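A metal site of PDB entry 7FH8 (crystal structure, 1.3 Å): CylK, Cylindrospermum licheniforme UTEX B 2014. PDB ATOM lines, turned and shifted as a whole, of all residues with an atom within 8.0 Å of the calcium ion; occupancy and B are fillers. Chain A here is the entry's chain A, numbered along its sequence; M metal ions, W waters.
O of Asp 559 sits at hydrogen-bond distance from N of Val 617, at 3.4 Å. The side-chain hydroxyl (OG1) of Thr 616 lies within hydrogen-bond range of the side-chain carboxylate (OD2) of Asp 559 (2.6 Å). O of Thr 615 lies within hydrogen-bond range of N of Asp 559, at 2.9 Å. NZ of Lys 377 is in salt-bridge range of OD1 of Asp 502 (3.5 Å). O of Asp 502 sits at hydrogen-bond distance from N of Thr 514 (3.0 Å).
The backbone carbonyl oxygen (O) of Ile 561 is bound to the calcium ion (2.3 Å). The calcium ion is bound by water W3, at 2.4 Å. OD1 of Asp 559 is bound to the calcium ion, at 2.4 Å. The calcium ion is bound by water W2, 2.4 Å away. OD2 of Asp 502 is bound to the calcium ion, 2.4 Å away. Water W4 binds the calcium ion. Water W1 is bound to the calcium ion, 2.5 Å away. The calcium ion has seven donor atoms within binding distance.
Water W1 lies within hydrogen-bond range of O of Val 617 (2.7 Å) and OD2 of Asp 559 (2.8 Å).
Three residues have an atom within 4 Å of the calcium ion: Asp 502, Asp 559 and Ile 561. The nearest printed residue that does not touch the calcium ion is Asp 562 (4.5 Å).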
ATOM      1  N   SER A 265     -14.035  -5.761 -36.632  1.00  0.00           N
ATOM      2  CA  SER A 265     -14.622  -6.318 -35.412  1.00  0.00           C
ATOM      3  C   SER A 265     -15.045  -7.756 -35.674  1.00  0.00           C
ATOM      4  O   SER A 265     -15.033  -8.240 -36.808  1.00  0.00           O
ATOM      5  CB  SER A 265     -15.815  -5.466 -34.937  1.00  0.00           C
ATOM      6  OG  SER A 265     -16.170  -5.792 -33.618  1.00  0.00           O
ATOM      7  N   SER A 266     -15.416  -8.419 -34.589  1.00  0.00           N
ATOM      8  CA  SER A 266     -15.836  -9.820 -34.641  1.00  0.00           C
ATOM      9  C   SER A 266     -16.640 -10.144 -33.399  1.00  0.00           C
ATOM     10  O   SER A 266     -16.599  -9.405 -32.402  1.00  0.00           O
ATOM     11  CB  SER A 266     -14.610 -10.747 -34.779  1.00  0.00           C
ATOM     12  OG  SER A 266     -13.743 -10.628 -33.665  1.00  0.00           O
ATOM     13  N   MET A 322     -19.254  -5.014 -33.213  1.00  0.00           N
ATOM     14  CA  MET A 322     -20.353  -5.967 -33.275  1.00  0.00           C
ATOM     15  C   MET A 322     -20.345  -6.832 -32.016  1.00  0.00           C
ATOM     16  O   MET A 322     -19.301  -7.071 -31.400  1.00  0.00           O
ATOM     17  CB  MET A 322     -20.310  -6.824 -34.540  1.00  0.00           C
ATOM     18  CG  MET A 322     -19.038  -7.618 -34.667  1.00  0.00           C
ATOM     19  SD  MET A 322     -18.695  -8.300 -36.323  1.00  0.00           S
ATOM     20  CE  MET A 322     -20.297  -8.871 -36.915  1.00  0.00           C
ATOM     21  N   LYS A 377     -17.749   1.440 -30.952  1.00  0.00           N
ATOM     22  CA  LYS A 377     -17.862   0.465 -29.880  1.00  0.00           C
ATOM     23  C   LYS A 377     -19.312   0.111 -29.601  1.00  0.00           C
ATOM     24  O   LYS A 377     -20.208   0.961 -29.680  1.00  0.00           O
ATOM     25  CB  LYS A 377     -17.219   0.985 -28.586  1.00  0.00           C
ATOM     26  CG  LYS A 377     -15.745   1.362 -28.733  1.00  0.00           C
ATOM     27  CD  LYS A 377     -14.875   0.138 -28.970  1.00  0.00           C
ATOM     28  CE  LYS A 377     -13.402   0.543 -29.074  1.00  0.00           C
ATOM     29  NZ  LYS A 377     -12.574  -0.578 -29.623  1.00  0.00           N
ATOM     30  N   ILE A 378     -19.530  -1.148 -29.217  1.00  0.00           N
ATOM     31  CA  ILE A 378     -20.848  -1.656 -28.868  1.00  0.00           C
ATOM     32  C   ILE A 378     -20.669  -2.793 -27.875  1.00  0.00           C
ATOM     33  O   ILE A 378     -19.657  -3.505 -27.900  1.00  0.00           O
ATOM     34  CB  ILE A 378     -21.602  -2.129 -30.132  1.00  0.00           C
ATOM     35  CG1 ILE A 378     -23.050  -2.520 -29.818  1.00  0.00           C
ATOM     36  CG2 ILE A 378     -20.878  -3.321 -30.803  1.00  0.00           C
ATOM     37  CD1 ILE A 378     -23.785  -2.982 -31.059  1.00  0.00           C
ATOM     38  N   GLY A 443     -14.086   2.473 -25.979  1.00  0.00           N
ATOM     39  CA  GLY A 443     -14.487   1.305 -25.218  1.00  0.00           C
ATOM     40  C   GLY A 443     -15.838   1.411 -24.566  1.00  0.00           C
ATOM     41  O   GLY A 443     -16.209   2.456 -24.039  1.00  0.00           O
ATOM     42  N   VAL A 444     -16.585   0.304 -24.558  1.00  0.00           N
ATOM     43  CA  VAL A 444     -17.827   0.200 -23.797  1.00  0.00           C
ATOM     44  C   VAL A 444     -17.976  -1.249 -23.342  1.00  0.00           C
ATOM     45  O   VAL A 444     -17.635  -2.178 -24.089  1.00  0.00           O
ATOM     46  CB  VAL A 444     -19.039   0.733 -24.611  1.00  0.00           C
ATOM     47  CG1 VAL A 444     -19.423  -0.203 -25.777  1.00  0.00           C
ATOM     48  CG2 VAL A 444     -20.226   0.999 -23.696  1.00  0.00           C
ATOM     49  N   ALA A 445     -18.453  -1.455 -22.106  1.00  0.00           N
ATOM     50  CA  ALA A 445     -18.593  -2.830 -21.629  1.00  0.00           C
ATOM     51  C   ALA A 445     -19.581  -2.868 -20.463  1.00  0.00           C
ATOM     52  O   ALA A 445     -19.407  -2.156 -19.475  1.00  0.00           O
ATOM     53  CB  ALA A 445     -17.245  -3.402 -21.150  1.00  0.00           C
ATOM     54  N   TRP A 501      -7.464   1.723 -26.545  1.00  0.00           N
ATOM     55  CA  TRP A 501      -8.177   1.176 -27.689  1.00  0.00           C
ATOM     56  C   TRP A 501      -9.461   0.423 -27.371  1.00  0.00           C
ATOM     57  O   TRP A 501     -10.380   0.450 -28.189  1.00  0.00           O
ATOM     58  CB  TRP A 501      -7.265   0.264 -28.524  1.00  0.00           C
ATOM     59  CG  TRP A 501      -6.350   1.026 -29.477  1.00  0.00           C
ATOM     60  CD1 TRP A 501      -4.983   1.069 -29.453  1.00  0.00           C
ATOM     61  CD2 TRP A 501      -6.752   1.770 -30.640  1.00  0.00           C
ATOM     62  NE1 TRP A 501      -4.510   1.834 -30.497  1.00  0.00           N
ATOM     63  CE2 TRP A 501      -5.571   2.261 -31.244  1.00  0.00           C
ATOM     64  CE3 TRP A 501      -7.990   2.079 -31.219  1.00  0.00           C
ATOM     65  CZ2 TRP A 501      -5.597   3.040 -32.408  1.00  0.00           C
ATOM     66  CZ3 TRP A 501      -8.020   2.856 -32.359  1.00  0.00           C
ATOM     67  CH2 TRP A 501      -6.836   3.326 -32.951  1.00  0.00           C
ATOM     68  N   ASP A 502      -9.530  -0.303 -26.241  1.00  0.00           N
ATOM     69  CA  ASP A 502     -10.717  -1.105 -25.979  1.00  0.00           C
ATOM     70  C   ASP A 502     -10.744  -1.478 -24.496  1.00  0.00           C
ATOM     71  O   ASP A 502      -9.721  -1.404 -23.806  1.00  0.00           O
ATOM     72  CB  ASP A 502     -10.723  -2.362 -26.871  1.00  0.00           C
ATOM     73  CG  ASP A 502     -12.058  -3.072 -26.912  1.00  0.00           C
ATOM     74  OD1 ASP A 502     -13.097  -2.410 -26.667  1.00  0.00           O
ATOM     75  OD2 ASP A 502     -12.058  -4.289 -27.215  1.00  0.00           O
ATOM     76  N   ILE A 503     -11.949  -1.833 -24.014  1.00  0.00           N
ATOM     77  CA  ILE A 503     -12.174  -2.227 -22.620  1.00  0.00           C
ATOM     78  C   ILE A 503     -13.130  -3.426 -22.588  1.00  0.00           C
ATOM     79  O   ILE A 503     -13.899  -3.651 -23.517  1.00  0.00           O
ATOM     80  CB  ILE A 503     -12.767  -1.091 -21.742  1.00  0.00           C
ATOM     81  CG1 ILE A 503     -14.253  -0.855 -22.032  1.00  0.00           C
ATOM     82  CG2 ILE A 503     -11.961   0.186 -21.885  1.00  0.00           C
ATOM     83  CD1 ILE A 503     -14.830   0.316 -21.232  1.00  0.00           C
ATOM     84  N   GLU A 504     -13.096  -4.179 -21.474  1.00  0.00           N
ATOM     85  CA  GLU A 504     -14.001  -5.305 -21.294  1.00  0.00           C
ATOM     86  C   GLU A 504     -14.067  -5.643 -19.805  1.00  0.00           C
ATOM     87  O   GLU A 504     -13.118  -5.378 -19.060  1.00  0.00           O
ATOM     88  CB  GLU A 504     -13.526  -6.528 -22.095  1.00  0.00           C
ATOM     89  CG  GLU A 504     -14.544  -7.673 -22.170  1.00  0.00           C
ATOM     90  CD  GLU A 504     -15.903  -7.171 -22.592  1.00  0.00           C
ATOM     91  OE1 GLU A 504     -16.126  -6.980 -23.799  1.00  0.00           O
ATOM     92  OE2 GLU A 504     -16.752  -6.929 -21.700  1.00  0.00           O
ATOM     93  N   THR A 514      -7.073  -1.728 -22.466  1.00  0.00           N
ATOM     94  CA  THR A 514      -5.784  -1.899 -23.125  1.00  0.00           C
ATOM     95  C   THR A 514      -5.500  -0.730 -24.063  1.00  0.00           C
ATOM     96  O   THR A 514      -6.421  -0.103 -24.605  1.00  0.00           O
ATOM     97  CB  THR A 514      -5.705  -3.257 -23.872  1.00  0.00           C
ATOM     98  OG1 THR A 514      -4.349  -3.509 -24.256  1.00  0.00           O
ATOM     99  CG2 THR A 514      -6.581  -3.259 -25.103  1.00  0.00           C
ATOM    100  N   LEU A 558      -7.630  -1.053 -32.364  1.00  0.00           N
ATOM    101  CA  LEU A 558      -9.078  -1.175 -32.532  1.00  0.00           C
ATOM    102  C   LEU A 558      -9.728  -2.083 -31.487  1.00  0.00           C
ATOM    103  O   LEU A 558      -9.740  -1.738 -30.308  1.00  0.00           O
ATOM    104  CB  LEU A 558      -9.471  -1.531 -33.989  1.00  0.00           C
ATOM    105  CG  LEU A 558      -9.202  -0.407 -35.006  1.00  0.00           C
ATOM    106  CD1 LEU A 558      -9.450  -0.867 -36.438  1.00  0.00           C
ATOM    107  CD2 LEU A 558     -10.095   0.795 -34.699  1.00  0.00           C
ATOM    108  N   ASP A 559     -10.269  -3.238 -31.904  1.00  0.00           N
ATOM    109  CA  ASP A 559     -11.001  -4.123 -30.988  1.00  0.00           C
ATOM    110  C   ASP A 559     -10.003  -5.043 -30.281  1.00  0.00           C
ATOM    111  O   ASP A 559      -9.971  -6.263 -30.476  1.00  0.00           O
ATOM    112  CB  ASP A 559     -12.051  -4.912 -31.751  1.00  0.00           C
ATOM    113  CG  ASP A 559     -12.887  -5.806 -30.849  1.00  0.00           C
ATOM    114  OD1 ASP A 559     -13.070  -5.450 -29.663  1.00  0.00           O
ATOM    115  OD2 ASP A 559     -13.347  -6.875 -31.336  1.00  0.00           O
ATOM    116  N   GLY A 560      -9.202  -4.424 -29.400  1.00  0.00           N
ATOM    117  CA  GLY A 560      -7.983  -5.032 -28.921  1.00  0.00           C
ATOM    118  C   GLY A 560      -8.071  -5.903 -27.691  1.00  0.00           C
ATOM    119  O   GLY A 560      -7.045  -6.465 -27.309  1.00  0.00           O
ATOM    120  N   ILE A 561      -9.228  -6.029 -27.028  1.00  0.00           N
ATOM    121  CA  ILE A 561      -9.348  -6.906 -25.861  1.00  0.00           C
ATOM    122  C   ILE A 561     -10.615  -7.730 -25.949  1.00  0.00           C
ATOM    123  O   ILE A 561     -11.651  -7.261 -26.442  1.00  0.00           O
ATOM    124  CB  ILE A 561      -9.318  -6.100 -24.527  1.00  0.00           C
ATOM    125  CG1 ILE A 561      -9.294  -7.019 -23.294  1.00  0.00           C
ATOM    126  CG2 ILE A 561     -10.497  -5.125 -24.418  1.00  0.00           C
ATOM    127  CD1 ILE A 561      -8.919  -6.285 -22.006  1.00  0.00           C
ATOM    128  N   ASP A 562     -10.555  -8.959 -25.428  1.00  0.00           N
ATOM    129  CA  ASP A 562     -11.749  -9.755 -25.162  1.00  0.00           C
ATOM    130  C   ASP A 562     -11.484 -10.569 -23.902  1.00  0.00           C
ATOM    131  O   ASP A 562     -10.333 -10.832 -23.563  1.00  0.00           O
ATOM    132  CB  ASP A 562     -12.112 -10.679 -26.328  1.00  0.00           C
ATOM    133  CG  ASP A 562     -13.487 -11.317 -26.164  1.00  0.00           C
ATOM    134  OD1 ASP A 562     -14.403 -10.613 -25.681  1.00  0.00           O
ATOM    135  OD2 ASP A 562     -13.643 -12.495 -26.526  1.00  0.00           O
ATOM    136  N   ILE A 563     -12.548 -10.972 -23.207  1.00  0.00           N
ATOM    137  CA  ILE A 563     -12.429 -11.753 -21.977  1.00  0.00           C
ATOM    138  C   ILE A 563     -13.384 -12.934 -22.058  1.00  0.00           C
ATOM    139  O   ILE A 563     -14.574 -12.746 -22.338  1.00  0.00           O
ATOM    140  CB  ILE A 563     -12.727 -10.888 -20.741  1.00  0.00           C
ATOM    141  CG1 ILE A 563     -11.716  -9.731 -20.675  1.00  0.00           C
ATOM    142  CG2 ILE A 563     -12.693 -11.748 -19.462  1.00  0.00           C
ATOM    143  CD1 ILE A 563     -11.892  -8.793 -19.484  1.00  0.00           C
ATOM    144  N   PHE A 570      -7.608 -11.620 -23.504  1.00  0.00           N
ATOM    145  CA  PHE A 570      -6.871 -11.731 -24.766  1.00  0.00           C
ATOM    146  C   PHE A 570      -6.697 -10.338 -25.341  1.00  0.00           C
ATOM    147  O   PHE A 570      -7.648  -9.545 -25.365  1.00  0.00           O
ATOM    148  CB  PHE A 570      -7.610 -12.630 -25.767  1.00  0.00           C
ATOM    149  CG  PHE A 570      -7.788 -14.028 -25.279  1.00  0.00           C
ATOM    150  CD1 PHE A 570      -6.819 -14.997 -25.520  1.00  0.00           C
ATOM    151  CD2 PHE A 570      -8.914 -14.388 -24.556  1.00  0.00           C
ATOM    152  CE1 PHE A 570      -6.992 -16.306 -25.076  1.00  0.00           C
ATOM    153  CE2 PHE A 570      -9.090 -15.691 -24.100  1.00  0.00           C
ATOM    154  CZ  PHE A 570      -8.113 -16.650 -24.368  1.00  0.00           C
ATOM    155  N   THR A 615      -6.961  -6.470 -35.902  1.00  0.00           N
ATOM    156  CA  THR A 615      -7.943  -5.450 -35.536  1.00  0.00           C
ATOM    157  C   THR A 615      -8.972  -5.950 -34.524  1.00  0.00           C
ATOM    158  O   THR A 615      -9.710  -5.127 -33.973  1.00  0.00           O
ATOM    159  CB  THR A 615      -8.705  -4.968 -36.775  1.00  0.00           C
ATOM    160  OG1 THR A 615      -9.377  -6.097 -37.352  1.00  0.00           O
ATOM    161  CG2 THR A 615      -7.772  -4.316 -37.807  1.00  0.00           C
ATOM    162  N   THR A 616      -9.046  -7.259 -34.265  1.00  0.00           N
ATOM    163  CA  THR A 616     -10.107  -7.761 -33.406  1.00  0.00           C
ATOM    164  C   THR A 616      -9.734  -9.150 -32.894  1.00  0.00           C
ATOM    165  O   THR A 616      -9.060  -9.926 -33.574  1.00  0.00           O
ATOM    166  CB  THR A 616     -11.461  -7.777 -34.169  1.00  0.00           C
ATOM    167  OG1 THR A 616     -12.500  -8.302 -33.342  1.00  0.00           O
ATOM    168  CG2 THR A 616     -11.375  -8.602 -35.447  1.00  0.00           C
ATOM    169  N   VAL A 617     -10.172  -9.442 -31.671  1.00  0.00           N
ATOM    170  CA  VAL A 617      -9.986 -10.740 -31.050  1.00  0.00           C
ATOM    171  C   VAL A 617     -11.288 -11.146 -30.358  1.00  0.00           C
ATOM    172  O   VAL A 617     -11.884 -10.340 -29.640  1.00  0.00           O
ATOM    173  CB  VAL A 617      -8.776 -10.741 -30.088  1.00  0.00           C
ATOM    174  CG1 VAL A 617      -8.910  -9.660 -28.999  1.00  0.00           C
ATOM    175  CG2 VAL A 617      -8.606 -12.101 -29.465  1.00  0.00           C
ATOM    176  N   THR A 618     -11.741 -12.373 -30.610  1.00  0.00           N
ATOM    177  CA  THR A 618     -12.923 -12.926 -29.944  1.00  0.00           C
ATOM    178  C   THR A 618     -12.634 -14.346 -29.511  1.00  0.00           C
ATOM    179  O   THR A 618     -12.222 -15.170 -30.325  1.00  0.00           O
ATOM    180  CB  THR A 618     -14.160 -12.947 -30.845  1.00  0.00           C
ATOM    181  OG1 THR A 618     -14.551 -11.617 -31.186  1.00  0.00           O
ATOM    182  CG2 THR A 618     -15.312 -13.574 -30.109  1.00  0.00           C
HETATM  183 CA    CA M   1     -13.457  -6.240 -27.457  1.00  0.00          CA
HETATM  184 MG    MG M   2     -16.498 -11.086 -25.144  1.00  0.00          MG
HETATM  185  O   HOH W   1     -13.505  -8.265 -28.927  1.00  0.00           O
HETATM  186  O   HOH W   2     -15.648  -5.857 -28.303  1.00  0.00           O
HETATM  187  O   HOH W   3     -14.533  -5.172 -25.632  1.00  0.00           O
HETATM  188  O   HOH W   4     -14.542  -7.869 -26.020  1.00  0.00           O
